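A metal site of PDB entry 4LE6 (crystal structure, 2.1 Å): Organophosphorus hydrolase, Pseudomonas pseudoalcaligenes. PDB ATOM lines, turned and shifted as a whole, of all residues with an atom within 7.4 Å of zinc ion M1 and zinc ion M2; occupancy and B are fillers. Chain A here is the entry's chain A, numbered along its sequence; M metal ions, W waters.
A ring nitrogen (ND1) of His 226 is in hydrogen-bond range of the side-chain carboxylate (OD1) of Asp 266 (2.7 Å). ND1 of His 294 is in hydrogen-bond range of O of Ala 88, 2.9 Å away. ND1 of His 144 lies within hydrogen-bond range of OD2 of Asp 104 (2.7 Å). A ring nitrogen (NE2) of His 230 is in hydrogen-bond range of the backbone NH (N) of Asp 247 (3.1 Å). A ring nitrogen (ND1) of His 139 lies within hydrogen-bond range of the side-chain hydroxyl of Thr 138.
Five residues have an atom within 4 Å of zinc ion M1: His 139, Asp 143, His 144, Asp 247 and His 294. The nearest printed residue that does not touch zinc ion M1 is His 226 (4.7 Å).
Five residues have an atom within 4 Å of zinc ion M2: His 139, His 141, His 144, His 226 and Asp 247.
Zinc ion M1 is bound by water W2 (1.8 Å), NE2 of His 294 (2.0 Å), NE2 of His 144 (2.1 Å), OD2 of Asp 247 (2.1 Å) and OD2 of Asp 143 (2.2 Å).
Zinc ion M2 is bound by a ring nitrogen (NE2) of His 226, a ring nitrogen (ND1) of His 141, water W2, a ring nitrogen (NE2) of His 139 and the side-chain carboxylate (OD2) of Asp 247. Zinc ion M2 has five donor atoms within binding distance.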
ATOM      1  N   ALA A  88     -31.550 -29.504   0.120  1.00  0.00           N
ATOM      2  CA  ALA A  88     -30.733 -30.702  -0.030  1.00  0.00           C
ATOM      3  C   ALA A  88     -29.914 -30.590  -1.294  1.00  0.00           C
ATOM      4  O   ALA A  88     -30.307 -29.902  -2.247  1.00  0.00           O
ATOM      5  CB  ALA A  88     -31.633 -31.919  -0.123  1.00  0.00           C
ATOM      6  N   VAL A  89     -28.772 -31.265  -1.292  1.00  0.00           N
ATOM      7  CA  VAL A  89     -27.941 -31.418  -2.484  1.00  0.00           C
ATOM      8  C   VAL A  89     -27.682 -32.914  -2.628  1.00  0.00           C
ATOM      9  O   VAL A  89     -27.097 -33.536  -1.742  1.00  0.00           O
ATOM     10  CB  VAL A  89     -26.618 -30.661  -2.328  1.00  0.00           C
ATOM     11  CG1 VAL A  89     -25.709 -30.899  -3.528  1.00  0.00           C
ATOM     12  CG2 VAL A  89     -26.868 -29.177  -2.135  1.00  0.00           C
ATOM     13  N   ASP A 104     -23.231 -36.153 -10.835  1.00  0.00           N
ATOM     14  CA  ASP A 104     -22.899 -35.075  -9.912  1.00  0.00           C
ATOM     15  C   ASP A 104     -22.127 -35.587  -8.717  1.00  0.00           C
ATOM     16  O   ASP A 104     -22.058 -36.791  -8.493  1.00  0.00           O
ATOM     17  CB  ASP A 104     -24.130 -34.258  -9.554  1.00  0.00           C
ATOM     18  CG  ASP A 104     -24.656 -33.459 -10.733  1.00  0.00           C
ATOM     19  OD1 ASP A 104     -23.884 -33.295 -11.711  1.00  0.00           O
ATOM     20  OD2 ASP A 104     -25.813 -32.976 -10.699  1.00  0.00           O
ATOM     21  N   PHE A 111     -18.934 -24.865  -0.281  1.00  0.00           N
ATOM     22  CA  PHE A 111     -19.986 -24.093   0.375  1.00  0.00           C
ATOM     23  C   PHE A 111     -20.021 -24.353   1.881  1.00  0.00           C
ATOM     24  O   PHE A 111     -21.058 -24.159   2.528  1.00  0.00           O
ATOM     25  CB  PHE A 111     -21.347 -24.442  -0.256  1.00  0.00           C
ATOM     26  CG  PHE A 111     -21.621 -23.750  -1.560  1.00  0.00           C
ATOM     27  CD1 PHE A 111     -21.169 -22.456  -1.780  1.00  0.00           C
ATOM     28  CD2 PHE A 111     -22.337 -24.378  -2.561  1.00  0.00           C
ATOM     29  CE1 PHE A 111     -21.413 -21.821  -2.974  1.00  0.00           C
ATOM     30  CE2 PHE A 111     -22.597 -23.733  -3.762  1.00  0.00           C
ATOM     31  CZ  PHE A 111     -22.126 -22.455  -3.963  1.00  0.00           C
ATOM     32  N   THR A 138     -24.332 -32.774 -14.475  1.00  0.00           N
ATOM     33  CA  THR A 138     -25.485 -32.101 -15.074  1.00  0.00           C
ATOM     34  C   THR A 138     -25.077 -30.696 -15.495  1.00  0.00           C
ATOM     35  O   THR A 138     -25.523 -30.197 -16.525  1.00  0.00           O
ATOM     36  CB  THR A 138     -26.717 -32.050 -14.145  1.00  0.00           C
ATOM     37  OG1 THR A 138     -26.365 -31.406 -12.914  1.00  0.00           O
ATOM     38  CG2 THR A 138     -27.182 -33.445 -13.859  1.00  0.00           C
ATOM     39  N   HIS A 139     -24.217 -30.063 -14.702  1.00  0.00           N
ATOM     40  CA  HIS A 139     -23.692 -28.729 -14.979  1.00  0.00           C
ATOM     41  C   HIS A 139     -22.527 -28.462 -14.043  1.00  0.00           C
ATOM     42  O   HIS A 139     -22.237 -29.260 -13.168  1.00  0.00           O
ATOM     43  CB  HIS A 139     -24.778 -27.630 -14.858  1.00  0.00           C
ATOM     44  CG  HIS A 139     -25.394 -27.508 -13.495  1.00  0.00           C
ATOM     45  ND1 HIS A 139     -26.001 -28.557 -12.850  1.00  0.00           N
ATOM     46  CD2 HIS A 139     -25.585 -26.423 -12.697  1.00  0.00           C
ATOM     47  CE1 HIS A 139     -26.504 -28.141 -11.693  1.00  0.00           C
ATOM     48  NE2 HIS A 139     -26.253 -26.850 -11.573  1.00  0.00           N
ATOM     49  N   LEU A 140     -21.867 -27.313 -14.223  1.00  0.00           N
ATOM     50  CA  LEU A 140     -20.579 -27.071 -13.571  1.00  0.00           C
ATOM     51  C   LEU A 140     -20.657 -26.254 -12.287  1.00  0.00           C
ATOM     52  O   LEU A 140     -19.629 -25.817 -11.741  1.00  0.00           O
ATOM     53  CB  LEU A 140     -19.629 -26.374 -14.558  1.00  0.00           C
ATOM     54  CG  LEU A 140     -19.276 -27.209 -15.785  1.00  0.00           C
ATOM     55  CD1 LEU A 140     -18.266 -26.469 -16.685  1.00  0.00           C
ATOM     56  CD2 LEU A 140     -18.744 -28.604 -15.377  1.00  0.00           C
ATOM     57  N   HIS A 141     -21.859 -26.079 -11.770  1.00  0.00           N
ATOM     58  CA  HIS A 141     -22.020 -25.351 -10.527  1.00  0.00           C
ATOM     59  C   HIS A 141     -21.241 -26.063  -9.412  1.00  0.00           C
ATOM     60  O   HIS A 141     -21.097 -27.285  -9.440  1.00  0.00           O
ATOM     61  CB  HIS A 141     -23.503 -25.235 -10.153  1.00  0.00           C
ATOM     62  CG  HIS A 141     -24.191 -24.036 -10.719  1.00  0.00           C
ATOM     63  ND1 HIS A 141     -25.573 -23.908 -10.726  1.00  0.00           N
ATOM     64  CD2 HIS A 141     -23.698 -22.892 -11.258  1.00  0.00           C
ATOM     65  CE1 HIS A 141     -25.901 -22.748 -11.264  1.00  0.00           C
ATOM     66  NE2 HIS A 141     -24.783 -22.115 -11.591  1.00  0.00           N
ATOM     67  N   PRO A 142     -20.734 -25.298  -8.430  1.00  0.00           N
ATOM     68  CA  PRO A 142     -19.933 -25.830  -7.327  1.00  0.00           C
ATOM     69  C   PRO A 142     -20.593 -27.017  -6.633  1.00  0.00           C
ATOM     70  O   PRO A 142     -19.904 -28.014  -6.363  1.00  0.00           O
ATOM     71  CB  PRO A 142     -19.847 -24.665  -6.350  1.00  0.00           C
ATOM     72  CG  PRO A 142     -20.123 -23.457  -7.138  1.00  0.00           C
ATOM     73  CD  PRO A 142     -21.066 -23.872  -8.213  1.00  0.00           C
ATOM     74  N   ASP A 143     -21.893 -26.928  -6.372  1.00  0.00           N
ATOM     75  CA  ASP A 143     -22.597 -27.973  -5.616  1.00  0.00           C
ATOM     76  C   ASP A 143     -22.807 -29.264  -6.420  1.00  0.00           C
ATOM     77  O   ASP A 143     -23.414 -30.230  -5.921  1.00  0.00           O
ATOM     78  CB  ASP A 143     -23.936 -27.471  -5.031  1.00  0.00           C
ATOM     79  CG  ASP A 143     -24.861 -26.832  -6.078  1.00  0.00           C
ATOM     80  OD1 ASP A 143     -24.378 -25.991  -6.855  1.00  0.00           O
ATOM     81  OD2 ASP A 143     -26.075 -27.162  -6.116  1.00  0.00           O
ATOM     82  N   HIS A 144     -22.285 -29.291  -7.643  1.00  0.00           N
ATOM     83  CA  HIS A 144     -22.327 -30.465  -8.505  1.00  0.00           C
ATOM     84  C   HIS A 144     -20.939 -30.934  -8.906  1.00  0.00           C
ATOM     85  O   HIS A 144     -20.701 -32.146  -9.077  1.00  0.00           O
ATOM     86  CB  HIS A 144     -23.182 -30.152  -9.749  1.00  0.00           C
ATOM     87  CG  HIS A 144     -24.572 -29.743  -9.395  1.00  0.00           C
ATOM     88  ND1 HIS A 144     -25.634 -30.619  -9.431  1.00  0.00           N
ATOM     89  CD2 HIS A 144     -25.071 -28.569  -8.935  1.00  0.00           C
ATOM     90  CE1 HIS A 144     -26.726 -30.009  -9.012  1.00  0.00           C
ATOM     91  NE2 HIS A 144     -26.414 -28.757  -8.716  1.00  0.00           N
ATOM     92  N   HIS A 226     -30.719 -23.083 -16.669  1.00  0.00           N
ATOM     93  CA  HIS A 226     -30.101 -22.908 -15.369  1.00  0.00           C
ATOM     94  C   HIS A 226     -28.611 -22.610 -15.579  1.00  0.00           C
ATOM     95  O   HIS A 226     -28.081 -21.679 -14.993  1.00  0.00           O
ATOM     96  CB  HIS A 226     -30.309 -24.156 -14.518  1.00  0.00           C
ATOM     97  CG  HIS A 226     -29.631 -24.110 -13.187  1.00  0.00           C
ATOM     98  ND1 HIS A 226     -29.978 -23.244 -12.182  1.00  0.00           N
ATOM     99  CD2 HIS A 226     -28.618 -24.868 -12.693  1.00  0.00           C
ATOM    100  CE1 HIS A 226     -29.206 -23.457 -11.125  1.00  0.00           C
ATOM    101  NE2 HIS A 226     -28.372 -24.440 -11.422  1.00  0.00           N
ATOM    102  N   THR A 227     -27.955 -23.407 -16.435  1.00  0.00           N
ATOM    103  CA  THR A 227     -26.727 -22.967 -17.098  1.00  0.00           C
ATOM    104  C   THR A 227     -26.886 -23.244 -18.594  1.00  0.00           C
ATOM    105  O   THR A 227     -27.714 -24.061 -18.999  1.00  0.00           O
ATOM    106  CB  THR A 227     -25.469 -23.707 -16.605  1.00  0.00           C
ATOM    107  OG1 THR A 227     -25.571 -25.096 -16.939  1.00  0.00           O
ATOM    108  CG2 THR A 227     -25.268 -23.550 -15.110  1.00  0.00           C
ATOM    109  N   HIS A 230     -26.653 -26.814 -19.335  1.00  0.00           N
ATOM    110  CA  HIS A 230     -27.274 -27.658 -18.334  1.00  0.00           C
ATOM    111  C   HIS A 230     -27.888 -28.895 -18.991  1.00  0.00           C
ATOM    112  O   HIS A 230     -28.614 -28.778 -19.971  1.00  0.00           O
ATOM    113  CB  HIS A 230     -28.348 -26.901 -17.565  1.00  0.00           C
ATOM    114  CG  HIS A 230     -28.939 -27.720 -16.485  1.00  0.00           C
ATOM    115  ND1 HIS A 230     -30.008 -28.568 -16.693  1.00  0.00           N
ATOM    116  CD2 HIS A 230     -28.574 -27.880 -15.191  1.00  0.00           C
ATOM    117  CE1 HIS A 230     -30.297 -29.185 -15.558  1.00  0.00           C
ATOM    118  NE2 HIS A 230     -29.442 -28.786 -14.640  1.00  0.00           N
ATOM    119  N   GLY A 246     -30.846 -32.985 -12.629  1.00  0.00           N
ATOM    120  CA  GLY A 246     -30.046 -31.856 -12.227  1.00  0.00           C
ATOM    121  C   GLY A 246     -30.892 -30.803 -11.530  1.00  0.00           C
ATOM    122  O   GLY A 246     -31.676 -31.113 -10.632  1.00  0.00           O
ATOM    123  N   ASP A 247     -30.716 -29.559 -11.947  1.00  0.00           N
ATOM    124  CA  ASP A 247     -31.326 -28.409 -11.322  1.00  0.00           C
ATOM    125  C   ASP A 247     -32.534 -27.853 -12.089  1.00  0.00           C
ATOM    126  O   ASP A 247     -32.739 -26.637 -12.154  1.00  0.00           O
ATOM    127  CB  ASP A 247     -30.253 -27.328 -11.125  1.00  0.00           C
ATOM    128  CG  ASP A 247     -29.317 -27.634  -9.973  1.00  0.00           C
ATOM    129  OD1 ASP A 247     -29.302 -28.797  -9.516  1.00  0.00           O
ATOM    130  OD2 ASP A 247     -28.585 -26.724  -9.534  1.00  0.00           O
ATOM    131  N   LEU A 249     -35.392 -27.847 -11.012  1.00  0.00           N
ATOM    132  CA  LEU A 249     -35.986 -26.954 -10.056  1.00  0.00           C
ATOM    133  C   LEU A 249     -35.268 -27.082  -8.736  1.00  0.00           C
ATOM    134  O   LEU A 249     -34.576 -28.070  -8.463  1.00  0.00           O
ATOM    135  CB  LEU A 249     -37.495 -27.162  -9.909  1.00  0.00           C
ATOM    136  CG  LEU A 249     -38.051 -28.499  -9.453  1.00  0.00           C
ATOM    137  CD1 LEU A 249     -38.199 -28.530  -7.920  1.00  0.00           C
ATOM    138  CD2 LEU A 249     -39.389 -28.729 -10.118  1.00  0.00           C
ATOM    139  N   LEU A 250     -35.419 -26.043  -7.948  1.00  0.00           N
ATOM    140  CA  LEU A 250     -34.672 -25.839  -6.733  1.00  0.00           C
ATOM    141  C   LEU A 250     -35.531 -25.950  -5.491  1.00  0.00           C
ATOM    142  O   LEU A 250     -35.014 -26.177  -4.405  1.00  0.00           O
ATOM    143  CB  LEU A 250     -34.071 -24.434  -6.781  1.00  0.00           C
ATOM    144  CG  LEU A 250     -32.630 -24.340  -6.305  1.00  0.00           C
ATOM    145  CD1 LEU A 250     -31.675 -24.390  -7.501  1.00  0.00           C
ATOM    146  CD2 LEU A 250     -32.492 -23.059  -5.519  1.00  0.00           C
ATOM    147  N   PHE A 263     -35.319 -18.995 -10.351  1.00  0.00           N
ATOM    148  CA  PHE A 263     -34.259 -18.869  -9.360  1.00  0.00           C
ATOM    149  C   PHE A 263     -33.274 -17.772  -9.788  1.00  0.00           C
ATOM    150  O   PHE A 263     -32.858 -17.725 -10.951  1.00  0.00           O
ATOM    151  CB  PHE A 263     -33.565 -20.223  -9.237  1.00  0.00           C
ATOM    152  CG  PHE A 263     -32.490 -20.287  -8.194  1.00  0.00           C
ATOM    153  CD1 PHE A 263     -32.725 -19.898  -6.894  1.00  0.00           C
ATOM    154  CD2 PHE A 263     -31.242 -20.790  -8.517  1.00  0.00           C
ATOM    155  CE1 PHE A 263     -31.719 -19.978  -5.939  1.00  0.00           C
ATOM    156  CE2 PHE A 263     -30.244 -20.887  -7.569  1.00  0.00           C
ATOM    157  CZ  PHE A 263     -30.482 -20.478  -6.290  1.00  0.00           C
ATOM    158  N   PHE A 265     -30.248 -17.385  -9.574  1.00  0.00           N
ATOM    159  CA  PHE A 265     -28.976 -17.857 -10.110  1.00  0.00           C
ATOM    160  C   PHE A 265     -29.110 -18.860 -11.268  1.00  0.00           C
ATOM    161  O   PHE A 265     -28.137 -19.511 -11.667  1.00  0.00           O
ATOM    162  CB  PHE A 265     -28.122 -18.409  -8.981  1.00  0.00           C
ATOM    163  CG  PHE A 265     -27.680 -17.352  -8.002  1.00  0.00           C
ATOM    164  CD1 PHE A 265     -27.061 -16.188  -8.434  1.00  0.00           C
ATOM    165  CD2 PHE A 265     -27.906 -17.507  -6.651  1.00  0.00           C
ATOM    166  CE1 PHE A 265     -26.675 -15.202  -7.534  1.00  0.00           C
ATOM    167  CE2 PHE A 265     -27.515 -16.535  -5.751  1.00  0.00           C
ATOM    168  CZ  PHE A 265     -26.899 -15.386  -6.199  1.00  0.00           C
ATOM    169  N   ASP A 266     -30.322 -18.964 -11.828  1.00  0.00           N
ATOM    170  CA  ASP A 266     -30.455 -19.457 -13.189  1.00  0.00           C
ATOM    171  C   ASP A 266     -29.693 -18.459 -14.083  1.00  0.00           C
ATOM    172  O   ASP A 266     -29.924 -17.253 -13.990  1.00  0.00           O
ATOM    173  CB  ASP A 266     -31.917 -19.513 -13.623  1.00  0.00           C
ATOM    174  CG  ASP A 266     -32.706 -20.587 -12.909  1.00  0.00           C
ATOM    175  OD1 ASP A 266     -32.134 -21.632 -12.551  1.00  0.00           O
ATOM    176  OD2 ASP A 266     -33.923 -20.387 -12.719  1.00  0.00           O
ATOM    177  N   ALA A 293     -31.460 -33.211  -7.986  1.00  0.00           N
ATOM    178  CA  ALA A 293     -30.345 -32.774  -7.161  1.00  0.00           C
ATOM    179  C   ALA A 293     -30.773 -31.973  -5.946  1.00  0.00           C
ATOM    180  O   ALA A 293     -30.080 -31.982  -4.918  1.00  0.00           O
ATOM    181  CB  ALA A 293     -29.376 -31.967  -7.989  1.00  0.00           C
ATOM    182  N   HIS A 294     -31.888 -31.259  -6.041  1.00  0.00           N
ATOM    183  CA  HIS A 294     -32.330 -30.410  -4.930  1.00  0.00           C
ATOM    184  C   HIS A 294     -33.721 -30.735  -4.416  1.00  0.00           C
ATOM    185  O   HIS A 294     -34.349 -29.935  -3.705  1.00  0.00           O
ATOM    186  CB  HIS A 294     -32.215 -28.934  -5.324  1.00  0.00           C
ATOM    187  CG  HIS A 294     -30.824 -28.527  -5.672  1.00  0.00           C
ATOM    188  ND1 HIS A 294     -29.767 -28.687  -4.796  1.00  0.00           N
ATOM    189  CD2 HIS A 294     -30.284 -28.032  -6.808  1.00  0.00           C
ATOM    190  CE1 HIS A 294     -28.656 -28.295  -5.371  1.00  0.00           C
ATOM    191  NE2 HIS A 294     -28.933 -27.895  -6.604  1.00  0.00           N
HETATM  192 ZN    ZN M   1     -27.424 -27.207  -7.806  1.00  0.00          ZN
HETATM  193 ZN    ZN M   2     -27.030 -25.280 -10.264  1.00  0.00          ZN
HETATM  194  O   HOH W   1     -28.162 -23.556  -8.173  1.00  0.00           O
HETATM  195  O   HOH W   2     -26.582 -25.636  -8.210  1.00  0.00           O
